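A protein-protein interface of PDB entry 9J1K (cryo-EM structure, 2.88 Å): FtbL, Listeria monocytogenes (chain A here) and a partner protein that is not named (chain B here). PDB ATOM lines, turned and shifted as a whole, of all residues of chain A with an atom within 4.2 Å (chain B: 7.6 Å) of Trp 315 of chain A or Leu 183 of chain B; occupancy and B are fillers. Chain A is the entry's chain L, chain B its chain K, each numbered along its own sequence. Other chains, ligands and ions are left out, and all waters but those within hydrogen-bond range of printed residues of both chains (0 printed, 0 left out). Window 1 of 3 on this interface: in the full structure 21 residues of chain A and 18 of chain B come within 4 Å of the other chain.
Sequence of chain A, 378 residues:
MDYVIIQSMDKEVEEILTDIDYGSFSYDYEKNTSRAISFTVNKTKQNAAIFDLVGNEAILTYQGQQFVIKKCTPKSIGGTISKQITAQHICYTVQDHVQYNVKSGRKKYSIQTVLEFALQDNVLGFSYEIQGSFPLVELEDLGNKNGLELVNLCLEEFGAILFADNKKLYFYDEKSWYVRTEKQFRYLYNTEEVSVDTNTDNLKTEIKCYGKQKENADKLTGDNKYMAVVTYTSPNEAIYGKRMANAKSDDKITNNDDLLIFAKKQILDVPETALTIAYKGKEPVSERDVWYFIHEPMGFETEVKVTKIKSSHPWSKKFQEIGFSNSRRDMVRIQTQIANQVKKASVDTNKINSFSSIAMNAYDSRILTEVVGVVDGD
Of the 8 printed residues of chain A, 4 touch a printed residue of chain B. Hydrophobic or aromatic side chains of chain A that line the printed part of chain B: Tyr 3 and Trp 315.
Trp 315 of chain A touches one residue of chain B. Leu 183 of chain B touches just these residues of chain A: Tyr 3 (3.6 Å), Thr 18 (3.7 Å) and Trp 315 (3.7 Å). Printed residues of chain B within 4 Å of Lys 317 of chain A: Glu 37. Printed residues of chain A within 4 Å of Glu 37 of chain B: Lys 317. The nearest residue of chain B that does not touch Trp 315 of chain A is Gln 53 of chain B (5.8 Å). The nearest printed residue of chain B that does not touch Thr 18 of chain A is Ile 226 of chain B (4.1 Å).
The backbone NH of Trp 315 of chain A lies close to a ring nitrogen (ND1) of His 313 of chain A (3.2 Å). N of Leu 183 of chain B is in hydrogen-bond range of OD1 of Asn 181 of chain B, 3.1 Å away.
NZ of Lys 317 of chain A lies within salt-bridge range of OE1 of Glu 37 of chain B (3.2 Å).
Among the printed residues, merely in contact across the chains: Tyr 3 of chain A with Leu 183 of chain B (3.6 Å), Trp 315 of chain A with Leu 183 of chain B (3.7 Å) and Thr 18 of chain A with Leu 183 of chain B (3.7 Å).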
ATOM      1  N   TYR A   3     -16.324  -7.231 -19.013  1.00  0.00           N
ATOM      2  CA  TYR A   3     -17.577  -7.125 -18.285  1.00  0.00           C
ATOM      3  C   TYR A   3     -17.313  -7.044 -16.784  1.00  0.00           C
ATOM      4  O   TYR A   3     -16.185  -7.204 -16.311  1.00  0.00           O
ATOM      5  CB  TYR A   3     -18.498  -8.300 -18.610  1.00  0.00           C
ATOM      6  CG  TYR A   3     -17.792  -9.620 -18.814  1.00  0.00           C
ATOM      7  CD1 TYR A   3     -17.364 -10.014 -20.074  1.00  0.00           C
ATOM      8  CD2 TYR A   3     -17.569 -10.481 -17.750  1.00  0.00           C
ATOM      9  CE1 TYR A   3     -16.724 -11.220 -20.266  1.00  0.00           C
ATOM     10  CE2 TYR A   3     -16.930 -11.690 -17.932  1.00  0.00           C
ATOM     11  CZ  TYR A   3     -16.509 -12.054 -19.191  1.00  0.00           C
ATOM     12  OH  TYR A   3     -15.870 -13.258 -19.378  1.00  0.00           O
ATOM     13  N   THR A  18     -24.857  -8.217 -15.974  1.00  0.00           N
ATOM     14  CA  THR A  18     -25.147  -8.001 -17.381  1.00  0.00           C
ATOM     15  C   THR A  18     -26.143  -6.859 -17.556  1.00  0.00           C
ATOM     16  O   THR A  18     -26.712  -6.339 -16.593  1.00  0.00           O
ATOM     17  CB  THR A  18     -25.688  -9.280 -18.024  1.00  0.00           C
ATOM     18  OG1 THR A  18     -25.718  -9.126 -19.448  1.00  0.00           O
ATOM     19  CG2 THR A  18     -27.090  -9.573 -17.522  1.00  0.00           C
ATOM     20  N   TYR A  22     -23.598   0.545 -20.809  1.00  0.00           N
ATOM     21  CA  TYR A  22     -22.195   0.844 -21.072  1.00  0.00           C
ATOM     22  C   TYR A  22     -21.987   2.264 -21.576  1.00  0.00           C
ATOM     23  O   TYR A  22     -20.871   2.786 -21.476  1.00  0.00           O
ATOM     24  CB  TYR A  22     -21.630  -0.157 -22.077  1.00  0.00           C
ATOM     25  CG  TYR A  22     -21.687  -1.588 -21.598  1.00  0.00           C
ATOM     26  CD1 TYR A  22     -20.900  -2.019 -20.540  1.00  0.00           C
ATOM     27  CD2 TYR A  22     -22.533  -2.509 -22.202  1.00  0.00           C
ATOM     28  CE1 TYR A  22     -20.952  -3.325 -20.097  1.00  0.00           C
ATOM     29  CE2 TYR A  22     -22.591  -3.816 -21.765  1.00  0.00           C
ATOM     30  CZ  TYR A  22     -21.798  -4.219 -20.714  1.00  0.00           C
ATOM     31  OH  TYR A  22     -21.854  -5.522 -20.277  1.00  0.00           O
ATOM     32  N   HIS A 313     -16.193   2.789 -21.358  1.00  0.00           N
ATOM     33  CA  HIS A 313     -16.189   1.362 -21.620  1.00  0.00           C
ATOM     34  C   HIS A 313     -15.745   1.103 -23.059  1.00  0.00           C
ATOM     35  O   HIS A 313     -16.018   1.906 -23.954  1.00  0.00           O
ATOM     36  CB  HIS A 313     -17.575   0.773 -21.382  1.00  0.00           C
ATOM     37  CG  HIS A 313     -17.580  -0.714 -21.216  1.00  0.00           C
ATOM     38  ND1 HIS A 313     -17.721  -1.581 -22.278  1.00  0.00           N
ATOM     39  CD2 HIS A 313     -17.457  -1.488 -20.112  1.00  0.00           C
ATOM     40  CE1 HIS A 313     -17.686  -2.825 -21.835  1.00  0.00           C
ATOM     41  NE2 HIS A 313     -17.527  -2.797 -20.524  1.00  0.00           N
ATOM     42  N   PRO A 314     -15.043  -0.006 -23.306  1.00  0.00           N
ATOM     43  CA  PRO A 314     -14.576  -0.287 -24.674  1.00  0.00           C
ATOM     44  C   PRO A 314     -15.696  -0.399 -25.691  1.00  0.00           C
ATOM     45  O   PRO A 314     -15.441  -0.215 -26.888  1.00  0.00           O
ATOM     46  CB  PRO A 314     -13.825  -1.615 -24.520  1.00  0.00           C
ATOM     47  CG  PRO A 314     -13.367  -1.615 -23.105  1.00  0.00           C
ATOM     48  CD  PRO A 314     -14.449  -0.928 -22.322  1.00  0.00           C
ATOM     49  N   TRP A 315     -16.920  -0.694 -25.265  1.00  0.00           N
ATOM     50  CA  TRP A 315     -18.062  -0.773 -26.165  1.00  0.00           C
ATOM     51  C   TRP A 315     -18.868   0.517 -26.211  1.00  0.00           C
ATOM     52  O   TRP A 315     -19.904   0.558 -26.880  1.00  0.00           O
ATOM     53  CB  TRP A 315     -18.979  -1.931 -25.757  1.00  0.00           C
ATOM     54  CG  TRP A 315     -18.272  -3.238 -25.568  1.00  0.00           C
ATOM     55  CD1 TRP A 315     -17.060  -3.599 -26.079  1.00  0.00           C
ATOM     56  CD2 TRP A 315     -18.735  -4.359 -24.808  1.00  0.00           C
ATOM     57  NE1 TRP A 315     -16.742  -4.875 -25.686  1.00  0.00           N
ATOM     58  CE2 TRP A 315     -17.755  -5.364 -24.905  1.00  0.00           C
ATOM     59  CE3 TRP A 315     -19.887  -4.611 -24.056  1.00  0.00           C
ATOM     60  CZ2 TRP A 315     -17.889  -6.600 -24.278  1.00  0.00           C
ATOM     61  CZ3 TRP A 315     -20.017  -5.837 -23.435  1.00  0.00           C
ATOM     62  CH2 TRP A 315     -19.024  -6.817 -23.549  1.00  0.00           C
ATOM     63  N   SER A 316     -18.424   1.565 -25.520  1.00  0.00           N
ATOM     64  CA  SER A 316     -19.211   2.780 -25.371  1.00  0.00           C
ATOM     65  C   SER A 316     -19.010   3.785 -26.498  1.00  0.00           C
ATOM     66  O   SER A 316     -19.728   4.789 -26.534  1.00  0.00           O
ATOM     67  CB  SER A 316     -18.888   3.457 -24.035  1.00  0.00           C
ATOM     68  OG  SER A 316     -19.421   4.767 -23.988  1.00  0.00           O
ATOM     69  N   LYS A 317     -18.029   3.566 -27.377  1.00  0.00           N
ATOM     70  CA  LYS A 317     -17.811   4.377 -28.575  1.00  0.00           C
ATOM     71  C   LYS A 317     -17.367   5.801 -28.250  1.00  0.00           C
ATOM     72  O   LYS A 317     -17.004   6.563 -29.152  1.00  0.00           O
ATOM     73  CB  LYS A 317     -19.078   4.391 -29.445  1.00  0.00           C
ATOM     74  CG  LYS A 317     -19.837   5.716 -29.466  1.00  0.00           C
ATOM     75  CD  LYS A 317     -21.260   5.550 -29.963  1.00  0.00           C
ATOM     76  CE  LYS A 317     -21.766   6.832 -30.605  1.00  0.00           C
ATOM     77  NZ  LYS A 317     -23.186   6.717 -31.033  1.00  0.00           N
ATOM     78  N   GLU B  37     -21.731   3.458 -35.420  1.00  0.00           N
ATOM     79  CA  GLU B  37     -21.508   4.446 -34.369  1.00  0.00           C
ATOM     80  C   GLU B  37     -20.381   5.365 -34.817  1.00  0.00           C
ATOM     81  O   GLU B  37     -19.206   5.147 -34.515  1.00  0.00           O
ATOM     82  CB  GLU B  37     -21.195   3.760 -33.046  1.00  0.00           C
ATOM     83  CG  GLU B  37     -22.094   2.570 -32.757  1.00  0.00           C
ATOM     84  CD  GLU B  37     -23.565   2.892 -32.951  1.00  0.00           C
ATOM     85  OE1 GLU B  37     -24.036   3.900 -32.384  1.00  0.00           O
ATOM     86  OE2 GLU B  37     -24.248   2.143 -33.679  1.00  0.00           O
ATOM     87  N   MET B  51     -18.751   0.196 -33.871  1.00  0.00           N
ATOM     88  CA  MET B  51     -19.263  -1.154 -34.053  1.00  0.00           C
ATOM     89  C   MET B  51     -20.658  -1.057 -34.653  1.00  0.00           C
ATOM     90  O   MET B  51     -21.536  -0.400 -34.084  1.00  0.00           O
ATOM     91  CB  MET B  51     -19.290  -1.916 -32.726  1.00  0.00           C
ATOM     92  CG  MET B  51     -18.027  -2.728 -32.365  1.00  0.00           C
ATOM     93  SD  MET B  51     -17.027  -3.699 -33.542  1.00  0.00           S
ATOM     94  CE  MET B  51     -18.128  -4.132 -34.893  1.00  0.00           C
ATOM     95  N   GLN B  53     -24.355  -1.609 -35.498  1.00  0.00           N
ATOM     96  CA  GLN B  53     -25.485  -2.118 -34.737  1.00  0.00           C
ATOM     97  C   GLN B  53     -26.733  -2.087 -35.608  1.00  0.00           C
ATOM     98  O   GLN B  53     -26.742  -1.515 -36.701  1.00  0.00           O
ATOM     99  CB  GLN B  53     -25.708  -1.311 -33.450  1.00  0.00           C
ATOM    100  CG  GLN B  53     -24.428  -0.941 -32.720  1.00  0.00           C
ATOM    101  CD  GLN B  53     -23.780  -2.118 -32.014  1.00  0.00           C
ATOM    102  OE1 GLN B  53     -24.241  -3.254 -32.112  1.00  0.00           O
ATOM    103  NE2 GLN B  53     -22.690  -1.849 -31.306  1.00  0.00           N
ATOM    104  N   VAL B 180     -23.626 -15.659 -31.855  1.00  0.00           N
ATOM    105  CA  VAL B 180     -24.479 -15.859 -30.688  1.00  0.00           C
ATOM    106  C   VAL B 180     -23.675 -15.503 -29.443  1.00  0.00           C
ATOM    107  O   VAL B 180     -22.715 -16.193 -29.092  1.00  0.00           O
ATOM    108  CB  VAL B 180     -25.010 -17.294 -30.616  1.00  0.00           C
ATOM    109  CG1 VAL B 180     -25.695 -17.536 -29.283  1.00  0.00           C
ATOM    110  CG2 VAL B 180     -25.966 -17.560 -31.767  1.00  0.00           C
ATOM    111  N   ASN B 181     -24.067 -14.425 -28.774  1.00  0.00           N
ATOM    112  CA  ASN B 181     -23.375 -13.940 -27.582  1.00  0.00           C
ATOM    113  C   ASN B 181     -24.402 -13.700 -26.486  1.00  0.00           C
ATOM    114  O   ASN B 181     -25.261 -12.807 -26.636  1.00  0.00           O
ATOM    115  CB  ASN B 181     -22.596 -12.665 -27.891  1.00  0.00           C
ATOM    116  CG  ASN B 181     -21.644 -12.275 -26.778  1.00  0.00           C
ATOM    117  OD1 ASN B 181     -21.673 -12.845 -25.688  1.00  0.00           O
ATOM    118  ND2 ASN B 181     -20.791 -11.296 -27.049  1.00  0.00           N
ATOM    119  N   PRO B 182     -24.360 -14.455 -25.386  1.00  0.00           N
ATOM    120  CA  PRO B 182     -25.320 -14.215 -24.297  1.00  0.00           C
ATOM    121  C   PRO B 182     -25.208 -12.831 -23.689  1.00  0.00           C
ATOM    122  O   PRO B 182     -26.187 -12.345 -23.110  1.00  0.00           O
ATOM    123  CB  PRO B 182     -24.975 -15.307 -23.276  1.00  0.00           C
ATOM    124  CG  PRO B 182     -23.575 -15.707 -23.598  1.00  0.00           C
ATOM    125  CD  PRO B 182     -23.440 -15.561 -25.081  1.00  0.00           C
ATOM    126  N   LEU B 183     -24.047 -12.180 -23.797  1.00  0.00           N
ATOM    127  CA  LEU B 183     -23.916 -10.811 -23.315  1.00  0.00           C
ATOM    128  C   LEU B 183     -24.782  -9.841 -24.104  1.00  0.00           C
ATOM    129  O   LEU B 183     -25.110  -8.764 -23.594  1.00  0.00           O
ATOM    130  CB  LEU B 183     -22.454 -10.372 -23.372  1.00  0.00           C
ATOM    131  CG  LEU B 183     -21.662 -10.565 -22.082  1.00  0.00           C
ATOM    132  CD1 LEU B 183     -20.256 -10.012 -22.230  1.00  0.00           C
ATOM    133  CD2 LEU B 183     -22.378  -9.911 -20.914  1.00  0.00           C
ATOM    134  N   MET B 184     -25.155 -10.194 -25.335  1.00  0.00           N
ATOM    135  CA  MET B 184     -26.052  -9.383 -26.149  1.00  0.00           C
ATOM    136  C   MET B 184     -27.507  -9.806 -26.005  1.00  0.00           C
ATOM    137  O   MET B 184     -28.295  -9.633 -26.943  1.00  0.00           O
ATOM    138  CB  MET B 184     -25.623  -9.437 -27.615  1.00  0.00           C
ATOM    139  CG  MET B 184     -24.124  -9.354 -27.819  1.00  0.00           C
ATOM    140  SD  MET B 184     -23.503  -7.666 -27.734  1.00  0.00           S
ATOM    141  CE  MET B 184     -22.052  -7.792 -28.774  1.00  0.00           C
ATOM    142  N   ARG B 185     -27.876 -10.365 -24.850  1.00  0.00           N
ATOM    143  CA  ARG B 185     -29.240 -10.817 -24.578  1.00  0.00           C
ATOM    144  C   ARG B 185     -29.692 -11.870 -25.586  1.00  0.00           C
ATOM    145  O   ARG B 185     -30.856 -11.912 -25.991  1.00  0.00           O
ATOM    146  CB  ARG B 185     -30.217  -9.641 -24.543  1.00  0.00           C
ATOM    147  CG  ARG B 185     -29.793  -8.520 -23.614  1.00  0.00           C
ATOM    148  CD  ARG B 185     -30.701  -7.317 -23.760  1.00  0.00           C
ATOM    149  NE  ARG B 185     -30.041  -6.227 -24.466  1.00  0.00           N
ATOM    150  CZ  ARG B 185     -30.413  -5.773 -25.654  1.00  0.00           C
ATOM    151  NH1 ARG B 185     -31.439  -6.298 -26.304  1.00  0.00           N
ATOM    152  NH2 ARG B 185     -29.742  -4.766 -26.203  1.00  0.00           N
ATOM    153  N   HIS B 186     -28.765 -12.727 -25.996  1.00  0.00           N
ATOM    154  CA  HIS B 186     -29.087 -13.856 -26.852  1.00  0.00           C
ATOM    155  C   HIS B 186     -29.401 -15.083 -26.006  1.00  0.00           C
ATOM    156  O   HIS B 186     -28.939 -15.222 -24.871  1.00  0.00           O
ATOM    157  CB  HIS B 186     -27.935 -14.163 -27.807  1.00  0.00           C
ATOM    158  CG  HIS B 186     -27.775 -13.160 -28.907  1.00  0.00           C
ATOM    159  ND1 HIS B 186     -26.579 -12.527 -29.168  1.00  0.00           N
ATOM    160  CD2 HIS B 186     -28.658 -12.685 -29.815  1.00  0.00           C
ATOM    161  CE1 HIS B 186     -26.733 -11.703 -30.188  1.00  0.00           C
ATOM    162  NE2 HIS B 186     -27.985 -11.780 -30.599  1.00  0.00           N
ATOM    163  N   ASN B 225     -27.433 -18.540 -20.714  1.00  0.00           N
ATOM    164  CA  ASN B 225     -27.002 -17.160 -20.905  1.00  0.00           C
ATOM    165  C   ASN B 225     -25.679 -16.910 -20.193  1.00  0.00           C
ATOM    166  O   ASN B 225     -24.632 -17.398 -20.630  1.00  0.00           O
ATOM    167  CB  ASN B 225     -28.078 -16.188 -20.418  1.00  0.00           C
ATOM    168  CG  ASN B 225     -29.471 -16.616 -20.828  1.00  0.00           C
ATOM    169  OD1 ASN B 225     -29.637 -17.478 -21.691  1.00  0.00           O
ATOM    170  ND2 ASN B 225     -30.480 -16.016 -20.210  1.00  0.00           N
ATOM    171  N   ILE B 226     -25.712 -16.160 -19.097  1.00  0.00           N
ATOM    172  CA  ILE B 226     -24.513 -15.843 -18.335  1.00  0.00           C
ATOM    173  C   ILE B 226     -24.582 -16.416 -16.920  1.00  0.00           C
ATOM    174  O   ILE B 226     -23.994 -15.859 -15.997  1.00  0.00           O
ATOM    175  CB  ILE B 226     -24.245 -14.329 -18.323  1.00  0.00           C
ATOM    176  CG1 ILE B 226     -25.554 -13.540 -18.199  1.00  0.00           C
ATOM    177  CG2 ILE B 226     -23.493 -13.914 -19.575  1.00  0.00           C
ATOM    178  CD1 ILE B 226     -26.119 -13.469 -16.801  1.00  0.00           C
ATOM    179  N   ILE B 243     -17.366 -16.866 -20.671  1.00  0.00           N
ATOM    180  CA  ILE B 243     -18.554 -17.281 -21.404  1.00  0.00           C
ATOM    181  C   ILE B 243     -18.157 -17.571 -22.842  1.00  0.00           C
ATOM    182  O   ILE B 243     -17.362 -16.837 -23.437  1.00  0.00           O
ATOM    183  CB  ILE B 243     -19.670 -16.216 -21.347  1.00  0.00           C
ATOM    184  CG1 ILE B 243     -19.150 -14.865 -21.839  1.00  0.00           C
ATOM    185  CG2 ILE B 243     -20.230 -16.106 -19.938  1.00  0.00           C
ATOM    186  CD1 ILE B 243     -20.018 -13.701 -21.446  1.00  0.00           C
ATOM    187  N   ILE B 244     -18.692 -18.643 -23.388  1.00  0.00           N
ATOM    188  CA  ILE B 244     -18.406 -19.023 -24.764  1.00  0.00           C
ATOM    189  C   ILE B 244     -19.417 -18.356 -25.684  1.00  0.00           C
ATOM    190  O   ILE B 244     -20.523 -17.989 -25.272  1.00  0.00           O
ATOM    191  CB  ILE B 244     -18.380 -20.562 -24.918  1.00  0.00           C
ATOM    192  CG1 ILE B 244     -19.650 -21.235 -24.375  1.00  0.00           C
ATOM    193  CG2 ILE B 244     -17.154 -21.140 -24.230  1.00  0.00           C
ATOM    194  CD1 ILE B 244     -20.896 -21.093 -25.225  1.00  0.00           C
ATOM    195  N   THR B 245     -19.026 -18.178 -26.940  1.00  0.00           N
ATOM    196  CA  THR B 245     -19.896 -17.619 -27.961  1.00  0.00           C
ATOM    197  C   THR B 245     -19.765 -18.448 -29.229  1.00  0.00           C
ATOM    198  O   THR B 245     -18.741 -19.091 -29.472  1.00  0.00           O
ATOM    199  CB  THR B 245     -19.566 -16.150 -28.258  1.00  0.00           C
ATOM    200  OG1 THR B 245     -18.174 -16.025 -28.570  1.00  0.00           O
ATOM    201  CG2 THR B 245     -19.891 -15.274 -27.060  1.00  0.00           C
